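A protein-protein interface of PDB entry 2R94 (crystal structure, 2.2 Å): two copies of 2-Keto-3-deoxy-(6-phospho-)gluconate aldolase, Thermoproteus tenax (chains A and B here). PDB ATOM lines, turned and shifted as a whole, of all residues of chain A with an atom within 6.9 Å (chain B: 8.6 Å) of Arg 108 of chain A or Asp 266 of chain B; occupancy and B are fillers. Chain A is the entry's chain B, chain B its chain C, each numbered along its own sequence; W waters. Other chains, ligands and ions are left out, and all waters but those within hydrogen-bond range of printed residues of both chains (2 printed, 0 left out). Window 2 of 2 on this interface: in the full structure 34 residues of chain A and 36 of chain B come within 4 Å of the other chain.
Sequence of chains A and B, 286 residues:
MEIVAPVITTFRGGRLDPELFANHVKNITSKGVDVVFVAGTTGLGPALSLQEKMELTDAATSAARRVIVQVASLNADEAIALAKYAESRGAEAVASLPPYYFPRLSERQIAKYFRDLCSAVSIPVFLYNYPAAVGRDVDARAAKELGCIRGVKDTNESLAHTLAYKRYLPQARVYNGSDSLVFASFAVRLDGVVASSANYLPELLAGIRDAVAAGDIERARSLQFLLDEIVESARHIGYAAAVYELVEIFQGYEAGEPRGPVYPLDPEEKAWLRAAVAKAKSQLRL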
ATOM      1  N   LEU A 105      -5.374  20.437  14.422  1.00  0.00           N
ATOM      2  CA  LEU A 105      -6.609  21.254  14.242  1.00  0.00           C
ATOM      3  C   LEU A 105      -6.744  22.316  15.300  1.00  0.00           C
ATOM      4  O   LEU A 105      -6.393  22.115  16.447  1.00  0.00           O
ATOM      5  CB  LEU A 105      -7.944  20.448  14.125  1.00  0.00           C
ATOM      6  CG  LEU A 105      -8.265  19.437  12.984  1.00  0.00           C
ATOM      7  CD1 LEU A 105      -9.690  19.027  12.966  1.00  0.00           C
ATOM      8  CD2 LEU A 105      -7.841  19.904  11.608  1.00  0.00           C
ATOM      9  N   SER A 106      -7.266  23.463  14.921  1.00  0.00           N
ATOM     10  CA  SER A 106      -7.201  24.593  15.803  1.00  0.00           C
ATOM     11  C   SER A 106      -8.534  24.708  16.528  1.00  0.00           C
ATOM     12  O   SER A 106      -9.552  24.228  16.041  1.00  0.00           O
ATOM     13  CB  SER A 106      -6.941  25.850  14.960  1.00  0.00           C
ATOM     14  OG  SER A 106      -8.125  26.180  14.225  1.00  0.00           O
ATOM     15  N   GLU A 107      -8.562  25.375  17.676  1.00  0.00           N
ATOM     16  CA  GLU A 107      -9.823  25.639  18.331  1.00  0.00           C
ATOM     17  C   GLU A 107     -10.800  26.378  17.449  1.00  0.00           C
ATOM     18  O   GLU A 107     -12.015  26.134  17.514  1.00  0.00           O
ATOM     19  CB  GLU A 107      -9.584  26.471  19.561  1.00  0.00           C
ATOM     20  CG  GLU A 107      -9.235  25.671  20.785  1.00  0.00           C
ATOM     21  CD  GLU A 107      -8.902  26.603  21.954  1.00  0.00           C
ATOM     22  OE1 GLU A 107      -9.583  27.677  22.085  1.00  0.00           O
ATOM     23  OE2 GLU A 107      -7.946  26.261  22.706  1.00  0.00           O
ATOM     24  N   ARG A 108     -10.293  27.292  16.628  1.00  0.00           N
ATOM     25  CA  ARG A 108     -11.155  28.068  15.718  1.00  0.00           C
ATOM     26  C   ARG A 108     -11.894  27.107  14.802  1.00  0.00           C
ATOM     27  O   ARG A 108     -13.110  27.236  14.545  1.00  0.00           O
ATOM     28  CB  ARG A 108     -10.271  29.032  14.892  1.00  0.00           C
ATOM     29  CG  ARG A 108     -10.728  30.505  14.730  1.00  0.00           C
ATOM     30  CD  ARG A 108     -11.161  30.882  13.235  1.00  0.00           C
ATOM     31  NE  ARG A 108     -10.253  30.318  12.212  1.00  0.00           N
ATOM     32  CZ  ARG A 108     -10.650  29.868  11.019  1.00  0.00           C
ATOM     33  NH1 ARG A 108     -11.938  29.946  10.660  1.00  0.00           N
ATOM     34  NH2 ARG A 108      -9.753  29.318  10.187  1.00  0.00           N
ATOM     35  N   GLN A 109     -11.172  26.115  14.300  1.00  0.00           N
ATOM     36  CA  GLN A 109     -11.738  25.188  13.343  1.00  0.00           C
ATOM     37  C   GLN A 109     -12.744  24.252  14.015  1.00  0.00           C
ATOM     38  O   GLN A 109     -13.765  23.918  13.425  1.00  0.00           O
ATOM     39  CB  GLN A 109     -10.612  24.376  12.682  1.00  0.00           C
ATOM     40  CG  GLN A 109      -9.704  25.143  11.700  1.00  0.00           C
ATOM     41  CD  GLN A 109      -8.516  24.280  11.251  1.00  0.00           C
ATOM     42  OE1 GLN A 109      -7.914  23.586  12.069  1.00  0.00           O
ATOM     43  NE2 GLN A 109      -8.188  24.304   9.965  1.00  0.00           N
ATOM     44  N   ILE A 110     -12.484  23.840  15.259  1.00  0.00           N
ATOM     45  CA  ILE A 110     -13.432  22.994  16.016  1.00  0.00           C
ATOM     46  C   ILE A 110     -14.676  23.783  16.405  1.00  0.00           C
ATOM     47  O   ILE A 110     -15.809  23.347  16.210  1.00  0.00           O
ATOM     48  CB  ILE A 110     -12.768  22.366  17.292  1.00  0.00           C
ATOM     49  CG1 ILE A 110     -11.630  21.401  16.860  1.00  0.00           C
ATOM     50  CG2 ILE A 110     -13.833  21.620  18.155  1.00  0.00           C
ATOM     51  CD1 ILE A 110     -10.631  21.130  18.004  1.00  0.00           C
ATOM     52  N   ALA A 111     -14.459  24.981  16.921  1.00  0.00           N
ATOM     53  CA  ALA A 111     -15.580  25.896  17.198  1.00  0.00           C
ATOM     54  C   ALA A 111     -16.436  26.127  15.961  1.00  0.00           C
ATOM     55  O   ALA A 111     -17.663  25.991  16.010  1.00  0.00           O
ATOM     56  CB  ALA A 111     -15.038  27.197  17.734  1.00  0.00           C
ATOM     57  N   LYS A 112     -15.820  26.467  14.828  1.00  0.00           N
ATOM     58  CA  LYS A 112     -16.615  26.683  13.599  1.00  0.00           C
ATOM     59  C   LYS A 112     -17.441  25.460  13.223  1.00  0.00           C
ATOM     60  O   LYS A 112     -18.612  25.574  12.842  1.00  0.00           O
ATOM     61  CB  LYS A 112     -15.723  27.066  12.437  1.00  0.00           C
ATOM     62  CG  LYS A 112     -16.512  27.382  11.178  1.00  0.00           C
ATOM     63  CD  LYS A 112     -15.592  28.025  10.073  1.00  0.00           C
ATOM     64  CE  LYS A 112     -16.280  28.085   8.673  1.00  0.00           C
ATOM     65  NZ  LYS A 112     -17.759  28.413   8.738  1.00  0.00           N
ATOM     66  N   TYR A 113     -16.852  24.269  13.319  1.00  0.00           N
ATOM     67  CA  TYR A 113     -17.593  23.067  12.939  1.00  0.00           C
ATOM     68  C   TYR A 113     -18.866  22.987  13.777  1.00  0.00           C
ATOM     69  O   TYR A 113     -19.960  22.812  13.254  1.00  0.00           O
ATOM     70  CB  TYR A 113     -16.738  21.812  13.128  1.00  0.00           C
ATOM     71  CG  TYR A 113     -17.496  20.507  12.928  1.00  0.00           C
ATOM     72  CD1 TYR A 113     -17.736  19.998  11.643  1.00  0.00           C
ATOM     73  CD2 TYR A 113     -17.944  19.765  14.018  1.00  0.00           C
ATOM     74  CE1 TYR A 113     -18.416  18.820  11.443  1.00  0.00           C
ATOM     75  CE2 TYR A 113     -18.642  18.550  13.826  1.00  0.00           C
ATOM     76  CZ  TYR A 113     -18.860  18.090  12.537  1.00  0.00           C
ATOM     77  OH  TYR A 113     -19.555  16.920  12.328  1.00  0.00           O
ATOM     78  N   ARG A 115     -20.431  25.315  15.565  1.00  0.00           N
ATOM     79  CA  ARG A 115     -21.337  26.462  15.346  1.00  0.00           C
ATOM     80  C   ARG A 115     -22.100  26.364  14.031  1.00  0.00           C
ATOM     81  O   ARG A 115     -23.305  26.612  14.004  1.00  0.00           O
ATOM     82  CB  ARG A 115     -20.617  27.788  15.538  1.00  0.00           C
ATOM     83  CG  ARG A 115     -20.298  28.011  17.006  1.00  0.00           C
ATOM     84  CD  ARG A 115     -19.303  29.113  17.159  1.00  0.00           C
ATOM     85  NE  ARG A 115     -18.939  29.275  18.561  1.00  0.00           N
ATOM     86  CZ  ARG A 115     -17.894  29.994  18.985  1.00  0.00           C
ATOM     87  NH1 ARG A 115     -17.119  30.603  18.087  1.00  0.00           N
ATOM     88  NH2 ARG A 115     -17.600  30.092  20.297  1.00  0.00           N
ATOM     89  N   HIS B 236       1.071  26.603  15.494  1.00  0.00           N
ATOM     90  CA  HIS B 236       0.389  27.488  16.401  1.00  0.00           C
ATOM     91  C   HIS B 236      -1.030  27.804  15.949  1.00  0.00           C
ATOM     92  O   HIS B 236      -1.925  27.934  16.772  1.00  0.00           O
ATOM     93  CB  HIS B 236       1.213  28.765  16.637  1.00  0.00           C
ATOM     94  CG  HIS B 236       0.647  29.641  17.703  1.00  0.00           C
ATOM     95  ND1 HIS B 236       0.814  29.372  19.050  1.00  0.00           N
ATOM     96  CD2 HIS B 236      -0.125  30.757  17.624  1.00  0.00           C
ATOM     97  CE1 HIS B 236       0.172  30.296  19.752  1.00  0.00           C
ATOM     98  NE2 HIS B 236      -0.404  31.147  18.913  1.00  0.00           N
ATOM     99  N   ILE B 237      -1.261  27.927  14.647  1.00  0.00           N
ATOM    100  CA  ILE B 237      -2.579  28.360  14.208  1.00  0.00           C
ATOM    101  C   ILE B 237      -3.389  27.269  13.556  1.00  0.00           C
ATOM    102  O   ILE B 237      -4.509  27.527  13.105  1.00  0.00           O
ATOM    103  CB  ILE B 237      -2.490  29.494  13.180  1.00  0.00           C
ATOM    104  CG1 ILE B 237      -1.329  29.229  12.237  1.00  0.00           C
ATOM    105  CG2 ILE B 237      -2.384  30.897  13.876  1.00  0.00           C
ATOM    106  CD1 ILE B 237      -1.499  29.977  10.908  1.00  0.00           C
ATOM    107  N   GLY B 238      -2.834  26.064  13.447  1.00  0.00           N
ATOM    108  CA  GLY B 238      -3.560  24.982  12.775  1.00  0.00           C
ATOM    109  C   GLY B 238      -2.721  24.528  11.601  1.00  0.00           C
ATOM    110  O   GLY B 238      -2.890  25.020  10.500  1.00  0.00           O
ATOM    111  N   ALA B 241      -4.369  23.578   7.867  1.00  0.00           N
ATOM    112  CA  ALA B 241      -4.668  24.736   7.024  1.00  0.00           C
ATOM    113  C   ALA B 241      -3.390  25.567   6.703  1.00  0.00           C
ATOM    114  O   ALA B 241      -3.281  26.177   5.660  1.00  0.00           O
ATOM    115  CB  ALA B 241      -5.729  25.609   7.677  1.00  0.00           C
ATOM    116  N   GLU B 245      -0.958  27.968   3.315  1.00  0.00           N
ATOM    117  CA  GLU B 245      -0.457  29.334   3.348  1.00  0.00           C
ATOM    118  C   GLU B 245       1.060  29.359   3.259  1.00  0.00           C
ATOM    119  O   GLU B 245       1.609  30.184   2.558  1.00  0.00           O
ATOM    120  CB  GLU B 245      -0.927  30.078   4.607  1.00  0.00           C
ATOM    121  CG  GLU B 245      -0.437  31.507   4.641  1.00  0.00           C
ATOM    122  CD  GLU B 245      -1.031  32.363   3.560  1.00  0.00           C
ATOM    123  OE1 GLU B 245      -1.922  31.876   2.817  1.00  0.00           O
ATOM    124  OE2 GLU B 245      -0.636  33.547   3.421  1.00  0.00           O
ATOM    125  N   PRO B 258      -7.966  24.084   2.123  1.00  0.00           N
ATOM    126  CA  PRO B 258      -8.448  22.805   2.661  1.00  0.00           C
ATOM    127  C   PRO B 258      -9.973  22.826   2.689  1.00  0.00           C
ATOM    128  O   PRO B 258     -10.565  23.740   2.186  1.00  0.00           O
ATOM    129  CB  PRO B 258      -7.881  22.768   4.079  1.00  0.00           C
ATOM    130  CG  PRO B 258      -7.773  24.185   4.484  1.00  0.00           C
ATOM    131  CD  PRO B 258      -7.484  24.978   3.205  1.00  0.00           C
ATOM    132  N   PRO B 261     -13.831  20.055   8.028  1.00  0.00           N
ATOM    133  CA  PRO B 261     -13.736  20.647   9.340  1.00  0.00           C
ATOM    134  C   PRO B 261     -12.321  21.224   9.368  1.00  0.00           C
ATOM    135  O   PRO B 261     -11.935  21.922  10.289  1.00  0.00           O
ATOM    136  CB  PRO B 261     -13.823  19.460  10.297  1.00  0.00           C
ATOM    137  CG  PRO B 261     -13.283  18.281   9.519  1.00  0.00           C
ATOM    138  CD  PRO B 261     -13.769  18.576   8.084  1.00  0.00           C
ATOM    139  N   VAL B 262     -11.521  20.938   8.356  1.00  0.00           N
ATOM    140  CA  VAL B 262     -10.231  21.575   8.320  1.00  0.00           C
ATOM    141  C   VAL B 262     -10.393  22.915   7.611  1.00  0.00           C
ATOM    142  O   VAL B 262      -9.987  23.056   6.458  1.00  0.00           O
ATOM    143  CB  VAL B 262      -9.227  20.719   7.562  1.00  0.00           C
ATOM    144  CG1 VAL B 262      -7.873  21.403   7.552  1.00  0.00           C
ATOM    145  CG2 VAL B 262      -9.166  19.288   8.171  1.00  0.00           C
ATOM    146  N   TYR B 263     -11.021  23.906   8.270  1.00  0.00           N
ATOM    147  CA  TYR B 263     -11.363  25.141   7.557  1.00  0.00           C
ATOM    148  C   TYR B 263     -10.101  25.910   7.229  1.00  0.00           C
ATOM    149  O   TYR B 263      -9.160  25.937   8.008  1.00  0.00           O
ATOM    150  CB  TYR B 263     -12.320  26.021   8.394  1.00  0.00           C
ATOM    151  CG  TYR B 263     -13.578  25.292   8.725  1.00  0.00           C
ATOM    152  CD1 TYR B 263     -14.611  25.212   7.816  1.00  0.00           C
ATOM    153  CD2 TYR B 263     -13.701  24.615   9.923  1.00  0.00           C
ATOM    154  CE1 TYR B 263     -15.776  24.489   8.106  1.00  0.00           C
ATOM    155  CE2 TYR B 263     -14.868  23.901  10.234  1.00  0.00           C
ATOM    156  CZ  TYR B 263     -15.899  23.864   9.330  1.00  0.00           C
ATOM    157  OH  TYR B 263     -17.041  23.123   9.645  1.00  0.00           O
ATOM    158  N   PRO B 264     -10.111  26.598   6.085  1.00  0.00           N
ATOM    159  CA  PRO B 264      -8.994  27.392   5.608  1.00  0.00           C
ATOM    160  C   PRO B 264      -8.665  28.493   6.623  1.00  0.00           C
ATOM    161  O   PRO B 264      -9.570  28.956   7.333  1.00  0.00           O
ATOM    162  CB  PRO B 264      -9.547  28.027   4.317  1.00  0.00           C
ATOM    163  CG  PRO B 264     -10.710  27.155   3.910  1.00  0.00           C
ATOM    164  CD  PRO B 264     -11.290  26.669   5.191  1.00  0.00           C
ATOM    165  N   LEU B 265      -7.412  28.948   6.663  1.00  0.00           N
ATOM    166  CA  LEU B 265      -7.042  30.032   7.560  1.00  0.00           C
ATOM    167  C   LEU B 265      -7.911  31.283   7.285  1.00  0.00           C
ATOM    168  O   LEU B 265      -8.370  31.509   6.140  1.00  0.00           O
ATOM    169  CB  LEU B 265      -5.562  30.369   7.420  1.00  0.00           C
ATOM    170  CG  LEU B 265      -4.536  29.315   7.840  1.00  0.00           C
ATOM    171  CD1 LEU B 265      -3.130  29.901   7.976  1.00  0.00           C
ATOM    172  CD2 LEU B 265      -4.923  28.703   9.178  1.00  0.00           C
ATOM    173  N   ASP B 266      -8.174  32.068   8.319  1.00  0.00           N
ATOM    174  CA  ASP B 266      -8.824  33.365   8.098  1.00  0.00           C
ATOM    175  C   ASP B 266      -7.733  34.438   7.885  1.00  0.00           C
ATOM    176  O   ASP B 266      -6.521  34.166   8.121  1.00  0.00           O
ATOM    177  CB  ASP B 266      -9.814  33.694   9.219  1.00  0.00           C
ATOM    178  CG  ASP B 266      -9.132  33.961  10.519  1.00  0.00           C
ATOM    179  OD1 ASP B 266      -7.905  34.226  10.458  1.00  0.00           O
ATOM    180  OD2 ASP B 266      -9.774  33.912  11.608  1.00  0.00           O
ATOM    181  N   PRO B 267      -8.116  35.628   7.337  1.00  0.00           N
ATOM    182  CA  PRO B 267      -7.117  36.703   7.069  1.00  0.00           C
ATOM    183  C   PRO B 267      -6.207  37.048   8.236  1.00  0.00           C
ATOM    184  O   PRO B 267      -4.997  37.241   8.046  1.00  0.00           O
ATOM    185  CB  PRO B 267      -7.991  37.884   6.675  1.00  0.00           C
ATOM    186  CG  PRO B 267      -9.124  37.185   5.880  1.00  0.00           C
ATOM    187  CD  PRO B 267      -9.454  36.008   6.820  1.00  0.00           C
ATOM    188  N   GLU B 268      -6.774  37.097   9.430  1.00  0.00           N
ATOM    189  CA  GLU B 268      -5.979  37.364  10.642  1.00  0.00           C
ATOM    190  C   GLU B 268      -4.905  36.286  10.862  1.00  0.00           C
ATOM    191  O   GLU B 268      -3.816  36.576  11.356  1.00  0.00           O
ATOM    192  CB  GLU B 268      -6.892  37.480  11.886  1.00  0.00           C
ATOM    193  CG  GLU B 268      -8.088  38.515  11.739  1.00  0.00           C
ATOM    194  CD  GLU B 268      -9.345  37.972  10.950  1.00  0.00           C
ATOM    195  OE1 GLU B 268      -9.488  38.264   9.702  1.00  0.00           O
ATOM    196  OE2 GLU B 268     -10.215  37.276  11.587  1.00  0.00           O
ATOM    197  N   GLU B 269      -5.234  35.032  10.520  1.00  0.00           N
ATOM    198  CA  GLU B 269      -4.354  33.889  10.833  1.00  0.00           C
ATOM    199  C   GLU B 269      -3.181  33.907   9.871  1.00  0.00           C
ATOM    200  O   GLU B 269      -2.023  33.702  10.271  1.00  0.00           O
ATOM    201  CB  GLU B 269      -5.137  32.564  10.760  1.00  0.00           C
ATOM    202  CG  GLU B 269      -5.779  32.178  12.098  1.00  0.00           C
ATOM    203  CD  GLU B 269      -6.909  31.154  11.986  1.00  0.00           C
ATOM    204  OE1 GLU B 269      -7.481  30.956  10.865  1.00  0.00           O
ATOM    205  OE2 GLU B 269      -7.278  30.564  13.046  1.00  0.00           O
ATOM    206  N   LYS B 270      -3.503  34.168   8.601  1.00  0.00           N
ATOM    207  CA  LYS B 270      -2.520  34.302   7.530  1.00  0.00           C
ATOM    208  C   LYS B 270      -1.541  35.448   7.769  1.00  0.00           C
ATOM    209  O   LYS B 270      -0.331  35.294   7.576  1.00  0.00           O
ATOM    210  CB  LYS B 270      -3.253  34.556   6.219  1.00  0.00           C
ATOM    211  CG  LYS B 270      -4.152  33.429   5.765  1.00  0.00           C
ATOM    212  CD  LYS B 270      -4.527  33.600   4.303  1.00  0.00           C
ATOM    213  CE  LYS B 270      -5.719  32.722   3.908  1.00  0.00           C
ATOM    214  NZ  LYS B 270      -6.220  33.073   2.541  1.00  0.00           N
ATOM    215  N   ALA B 271      -2.071  36.606   8.176  1.00  0.00           N
ATOM    216  CA  ALA B 271      -1.248  37.775   8.418  1.00  0.00           C
ATOM    217  C   ALA B 271      -0.318  37.410   9.504  1.00  0.00           C
ATOM    218  O   ALA B 271       0.884  37.749   9.459  1.00  0.00           O
ATOM    219  CB  ALA B 271      -2.131  38.983   8.863  1.00  0.00           C
ATOM    220  N   TRP B 272      -0.853  36.718  10.514  1.00  0.00           N
ATOM    221  CA  TRP B 272      -0.028  36.375  11.688  1.00  0.00           C
ATOM    222  C   TRP B 272       1.071  35.426  11.258  1.00  0.00           C
ATOM    223  O   TRP B 272       2.273  35.573  11.606  1.00  0.00           O
ATOM    224  CB  TRP B 272      -0.880  35.682  12.766  1.00  0.00           C
ATOM    225  CG  TRP B 272      -0.042  35.333  13.935  1.00  0.00           C
ATOM    226  CD1 TRP B 272       0.240  36.141  15.024  1.00  0.00           C
ATOM    227  CD2 TRP B 272       0.685  34.107  14.137  1.00  0.00           C
ATOM    228  NE1 TRP B 272       1.083  35.471  15.896  1.00  0.00           N
ATOM    229  CE2 TRP B 272       1.381  34.232  15.371  1.00  0.00           C
ATOM    230  CE3 TRP B 272       0.815  32.917  13.401  1.00  0.00           C
ATOM    231  CZ2 TRP B 272       2.177  33.209  15.881  1.00  0.00           C
ATOM    232  CZ3 TRP B 272       1.612  31.902  13.905  1.00  0.00           C
ATOM    233  CH2 TRP B 272       2.288  32.056  15.128  1.00  0.00           C
ATOM    234  N   LEU B 273       0.658  34.406  10.517  1.00  0.00           N
ATOM    235  CA  LEU B 273       1.624  33.437   9.991  1.00  0.00           C
ATOM    236  C   LEU B 273       2.686  34.132   9.131  1.00  0.00           C
ATOM    237  O   LEU B 273       3.895  33.960   9.360  1.00  0.00           O
ATOM    238  CB  LEU B 273       0.878  32.378   9.174  1.00  0.00           C
ATOM    239  CG  LEU B 273       1.763  31.239   8.664  1.00  0.00           C
ATOM    240  CD1 LEU B 273       2.445  30.568   9.859  1.00  0.00           C
ATOM    241  CD2 LEU B 273       0.910  30.268   7.855  1.00  0.00           C
ATOM    242  N   ARG B 274       2.251  34.879   8.114  1.00  0.00           N
ATOM    243  CA  ARG B 274       3.203  35.607   7.266  1.00  0.00           C
ATOM    244  C   ARG B 274       4.229  36.322   8.145  1.00  0.00           C
ATOM    245  O   ARG B 274       5.447  36.193   7.944  1.00  0.00           O
ATOM    246  CB  ARG B 274       2.501  36.646   6.367  1.00  0.00           C
ATOM    247  CG  ARG B 274       1.563  36.061   5.290  1.00  0.00           C
ATOM    248  CD  ARG B 274       1.813  36.653   3.846  1.00  0.00           C
ATOM    249  NE  ARG B 274       0.713  36.336   2.904  1.00  0.00           N
ATOM    250  CZ  ARG B 274      -0.555  36.748   3.092  1.00  0.00           C
ATOM    251  NH1 ARG B 274      -0.844  37.462   4.188  1.00  0.00           N
ATOM    252  NH2 ARG B 274      -1.536  36.442   2.209  1.00  0.00           N
HETATM  253  O   HOH W   1      -7.315  27.757  12.173  1.00  0.00           O
HETATM  254  O   HOH W   2      -5.533  23.227  10.586  1.00  0.00           O
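The side-chain hydroxyl (OG) of Ser 106 of chain A lies close to the backbone NH (N) of Arg 108 of chain A (3.4 Å). The backbone NH (N) of Ser 106 of chain A is in hydrogen-bond range of the side-chain amide oxygen (OE1) of Gln 109 of chain A, 2.9 Å away. N of Glu 268 of chain B sits close to OD1 of Asp 266 of chain B (3.3 Å). The backbone NH (N) of Glu 269 of chain B is in hydrogen-bond range of the side-chain carboxylate (OD1) of Asp 266 of chain B, 2.8 Å away.
The guanidinium group (NH2) of Arg 108 of chain A sits at hydrogen-bond distance from the backbone carbonyl oxygen (O) of Pro 264 of chain B, 2.9 Å away. The side-chain carboxylate (OD2) of Asp 266 of chain B lies within salt-bridge range of the guanidinium group (NE) of Arg 108 of chain A, 3.7 Å away. OE1 of Glu 269 of chain B lies within salt-bridge range of NH2 of Arg 108 of chain A, 2.9 Å away. The side-chain amide nitrogen of Gln 109 of chain A lies within hydrogen-bond range of the backbone carbonyl oxygen of Tyr 263 of chain B.
Of the 20 printed residues of chain B, 9 touch a printed residue of chain A. Hydrophobic or aromatic side chains of chain B within 4 Å of the printed part of chain A: Ala 241, Val 262 and Tyr 263. Hydrophobic or aromatic side chains of chain A that line the printed part of chain B: Leu 105 and Tyr 113. Among the printed residues, 12 pairs touch across the chains.
Water W1 lies within hydrogen-bond range of OG of Ser 106 of chain A (2.7 Å), OE2 of Glu 269 of chain B (2.9 Å) and O of Ile 237 of chain B (3.0 Å). Water W2 lies within hydrogen-bond range of OE1 of Gln 109 of chain A, N of Ala 241 of chain B and O of Gly 238 of chain B.
Among the printed residues, merely in contact across the chains: Leu 105 of chain A with Val 262 of chain B, Ser 106 of chain A with Ile 237 of chain B, Arg 108 of chain A with Leu 265 of chain B, Gln 109 of chain A with Ala 241 of chain B, Gln 109 of chain A with Pro 261 of chain B, Gln 109 of chain A with Val 262 of chain B, Lys 112 of chain A with Tyr 263 of chain B and Tyr 113 of chain A with Tyr 263 of chain B.
No position is printed for both chains.
Arg 108 of chain A touches just these residues of chain B: Pro 264 (2.9 Å), Leu 265 (3.8 Å), Asp 266 (3.7 Å) and Glu 269 (2.9 Å). Printed residues of chain B within 4 Å of Tyr 113 of chain A: Tyr 263 (3.3 Å). Of the printed residues of chain B, Gln 109 of chain A touches Ala 241, Pro 261, Val 262 and Tyr 263. Printed residues of chain B within 4 Å of Ser 106 of chain A: Ile 237 (3.5 Å). The nearest printed residue of chain A that does not touch Asp 266 of chain B is Gln 109 of chain A (7.9 Å).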
